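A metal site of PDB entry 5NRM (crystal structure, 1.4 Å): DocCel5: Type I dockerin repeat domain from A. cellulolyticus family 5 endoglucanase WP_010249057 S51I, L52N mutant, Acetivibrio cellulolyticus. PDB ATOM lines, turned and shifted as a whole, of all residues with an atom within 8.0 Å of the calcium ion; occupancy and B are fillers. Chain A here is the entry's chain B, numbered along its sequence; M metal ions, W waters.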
ATOM      1  N   VAL A   5       2.312 -28.329   8.762  1.00  0.00           N
ATOM      2  CA  VAL A   5       3.697 -27.976   9.071  1.00  0.00           C
ATOM      3  C   VAL A   5       4.111 -28.094  10.537  1.00  0.00           C
ATOM      4  O   VAL A   5       5.276 -28.271  10.759  1.00  0.00           O
ATOM      5  CB  VAL A   5       4.079 -26.543   8.491  1.00  0.00           C
ATOM      6  CG1 VAL A   5       3.827 -26.484   7.004  1.00  0.00           C
ATOM      7  CG2 VAL A   5       3.380 -25.440   9.198  1.00  0.00           C
ATOM      8  N   TYR A  22       7.940 -18.504   8.324  1.00  0.00           N
ATOM      9  CA  TYR A  22       9.002 -19.059   7.474  1.00  0.00           C
ATOM     10  C   TYR A  22       9.292 -18.094   6.310  1.00  0.00           C
ATOM     11  O   TYR A  22      10.463 -17.724   6.016  1.00  0.00           O
ATOM     12  CB  TYR A  22       8.569 -20.427   6.937  1.00  0.00           C
ATOM     13  CG  TYR A  22       9.617 -21.169   6.120  1.00  0.00           C
ATOM     14  CD1 TYR A  22       9.791 -20.885   4.770  1.00  0.00           C
ATOM     15  CD2 TYR A  22      10.352 -22.222   6.683  1.00  0.00           C
ATOM     16  CE1 TYR A  22      10.721 -21.584   4.006  1.00  0.00           C
ATOM     17  CE2 TYR A  22      11.279 -22.932   5.927  1.00  0.00           C
ATOM     18  CZ  TYR A  22      11.449 -22.595   4.602  1.00  0.00           C
ATOM     19  OH  TYR A  22      12.328 -23.270   3.801  1.00  0.00           O
ATOM     20  N   LYS A  28      13.246 -20.860  10.575  1.00  0.00           N
ATOM     21  CA  LYS A  28      14.052 -21.654   9.631  1.00  0.00           C
ATOM     22  C   LYS A  28      13.618 -23.100   9.368  1.00  0.00           C
ATOM     23  O   LYS A  28      13.895 -23.669   8.300  1.00  0.00           O
ATOM     24  CB  LYS A  28      15.553 -21.658  10.058  1.00  0.00           C
ATOM     25  CG  LYS A  28      16.313 -20.458   9.547  1.00  0.00           C
ATOM     26  CD  LYS A  28      15.702 -19.178  10.099  1.00  0.00           C
ATOM     27  CE  LYS A  28      16.566 -17.943   9.873  1.00  0.00           C
ATOM     28  NZ  LYS A  28      15.998 -16.882  10.757  1.00  0.00           N
ATOM     29  N   ASP A  29      12.932 -23.687  10.337  1.00  0.00           N
ATOM     30  CA  ASP A  29      12.647 -25.084  10.285  1.00  0.00           C
ATOM     31  C   ASP A  29      11.213 -25.266  10.789  1.00  0.00           C
ATOM     32  O   ASP A  29      10.890 -24.721  11.830  1.00  0.00           O
ATOM     33  CB  ASP A  29      13.611 -25.789  11.283  1.00  0.00           C
ATOM     34  CG  ASP A  29      13.780 -27.273  10.998  1.00  0.00           C
ATOM     35  OD1 ASP A  29      12.978 -27.913  10.277  1.00  0.00           O
ATOM     36  OD2 ASP A  29      14.796 -27.833  11.498  1.00  0.00           O
ATOM     37  N   PHE A  30      10.401 -26.039  10.090  1.00  0.00           N
ATOM     38  CA  PHE A  30       9.113 -26.407  10.614  1.00  0.00           C
ATOM     39  C   PHE A  30       9.259 -27.593  11.601  1.00  0.00           C
ATOM     40  O   PHE A  30      10.152 -28.417  11.477  1.00  0.00           O
ATOM     41  CB  PHE A  30       8.186 -26.857   9.478  1.00  0.00           C
ATOM     42  CG  PHE A  30       7.768 -25.747   8.518  1.00  0.00           C
ATOM     43  CD1 PHE A  30       7.219 -24.570   8.989  1.00  0.00           C
ATOM     44  CD2 PHE A  30       7.898 -25.927   7.153  1.00  0.00           C
ATOM     45  CE1 PHE A  30       6.785 -23.604   8.107  1.00  0.00           C
ATOM     46  CE2 PHE A  30       7.460 -24.973   6.280  1.00  0.00           C
ATOM     47  CZ  PHE A  30       6.923 -23.804   6.768  1.00  0.00           C
ATOM     48  N   PRO A  31       8.305 -27.695  12.546  1.00  0.00           N
ATOM     49  CA  PRO A  31       8.258 -28.872  13.397  1.00  0.00           C
ATOM     50  C   PRO A  31       8.075 -30.134  12.643  1.00  0.00           C
ATOM     51  O   PRO A  31       8.519 -31.193  13.101  1.00  0.00           O
ATOM     52  CB  PRO A  31       7.052 -28.658  14.277  1.00  0.00           C
ATOM     53  CG  PRO A  31       6.905 -27.218  14.311  1.00  0.00           C
ATOM     54  CD  PRO A  31       7.357 -26.653  12.987  1.00  0.00           C
ATOM     55  N   ALA A  32       7.405 -30.085  11.503  1.00  0.00           N
ATOM     56  CA  ALA A  32       7.354 -31.263  10.680  1.00  0.00           C
ATOM     57  C   ALA A  32       8.794 -31.805  10.375  1.00  0.00           C
ATOM     58  O   ALA A  32       9.837 -31.107  10.154  1.00  0.00           O
ATOM     59  CB  ALA A  32       6.552 -31.042   9.370  1.00  0.00           C
ATOM     60  N   GLU A  33       8.769 -33.107  10.344  1.00  0.00           N
ATOM     61  CA  GLU A  33       9.904 -33.925  10.099  1.00  0.00           C
ATOM     62  C   GLU A  33      10.494 -33.574   8.716  1.00  0.00           C
ATOM     63  O   GLU A  33      11.752 -33.462   8.532  1.00  0.00           O
ATOM     64  CB  GLU A  33       9.464 -35.413  10.197  1.00  0.00           C
ATOM     65  CG  GLU A  33      10.220 -36.285  11.243  1.00  0.00           C
ATOM     66  CD  GLU A  33       9.787 -36.091  12.722  1.00  0.00           C
ATOM     67  OE1 GLU A  33       8.825 -36.792  13.243  1.00  0.00           O
ATOM     68  OE2 GLU A  33      10.450 -35.219  13.377  1.00  0.00           O
ATOM     69  N   ASP A  34       9.603 -33.382   7.753  1.00  0.00           N
ATOM     70  CA  ASP A  34      10.001 -33.042   6.382  1.00  0.00           C
ATOM     71  C   ASP A  34       9.348 -31.700   5.976  1.00  0.00           C
ATOM     72  O   ASP A  34       8.179 -31.675   5.654  1.00  0.00           O
ATOM     73  CB  ASP A  34       9.526 -34.179   5.528  1.00  0.00           C
ATOM     74  CG  ASP A  34       9.888 -34.032   4.075  1.00  0.00           C
ATOM     75  OD1 ASP A  34      10.445 -32.976   3.621  1.00  0.00           O
ATOM     76  OD2 ASP A  34       9.687 -35.059   3.379  1.00  0.00           O
ATOM     77  N   ASP A  35      10.095 -30.607   6.043  1.00  0.00           N
ATOM     78  CA  ASP A  35       9.550 -29.284   5.788  1.00  0.00           C
ATOM     79  C   ASP A  35       8.989 -29.292   4.362  1.00  0.00           C
ATOM     80  O   ASP A  35       7.940 -28.673   4.104  1.00  0.00           O
ATOM     81  CB  ASP A  35      10.604 -28.164   5.908  1.00  0.00           C
ATOM     82  CG  ASP A  35      11.074 -27.910   7.342  1.00  0.00           C
ATOM     83  OD1 ASP A  35      10.733 -28.633   8.242  1.00  0.00           O
ATOM     84  OD2 ASP A  35      11.763 -26.923   7.573  1.00  0.00           O
ATOM     85  N   ILE A  36       9.664 -29.933   3.396  1.00  0.00           N
ATOM     86  CA  ILE A  36       9.144 -29.833   2.025  1.00  0.00           C
ATOM     87  C   ILE A  36       7.827 -30.574   1.797  1.00  0.00           C
ATOM     88  O   ILE A  36       6.874 -29.975   1.239  1.00  0.00           O
ATOM     89  CB  ILE A  36      10.194 -30.254   0.959  1.00  0.00           C
ATOM     90  CG1 ILE A  36      11.530 -29.529   1.184  1.00  0.00           C
ATOM     91  CG2 ILE A  36       9.757 -29.930  -0.465  1.00  0.00           C
ATOM     92  CD1 ILE A  36      11.527 -27.997   1.215  1.00  0.00           C
ATOM     93  N   ALA A  38       5.643 -31.227   4.014  1.00  0.00           N
ATOM     94  CA  ALA A  38       4.619 -30.478   4.726  1.00  0.00           C
ATOM     95  C   ALA A  38       4.294 -29.130   4.118  1.00  0.00           C
ATOM     96  O   ALA A  38       3.133 -28.731   4.132  1.00  0.00           O
ATOM     97  CB  ALA A  38       5.016 -30.314   6.192  1.00  0.00           C
HETATM   98 CA    CA M   1      11.488 -29.569  10.115  1.00  0.00          CA
HETATM   99  O   HOH W   1      13.194 -30.424   8.784  1.00  0.00           O
HETATM  100  O   HOH W   2      12.213 -30.812  12.072  1.00  0.00           O
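The backbone carbonyl oxygen (O) of Val 5 is in hydrogen-bond range of the backbone NH (N) of Ala 32 (2.9 Å).
The calcium ion is bound by OD1 of Asp 35 (2.2 Å), O of Phe 30 (2.2 Å), OD1 of Asp 29 (2.2 Å), O of Ala 32 (2.3 Å), water W1 (2.3 Å) and water W2 (2.4 Å).
Within 4 Å of the calcium ion: Asp 29, Phe 30, Ala 32 and Asp 35.
The nearest printed residue that does not touch the calcium ion is Glu 33 (4.2 Å).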
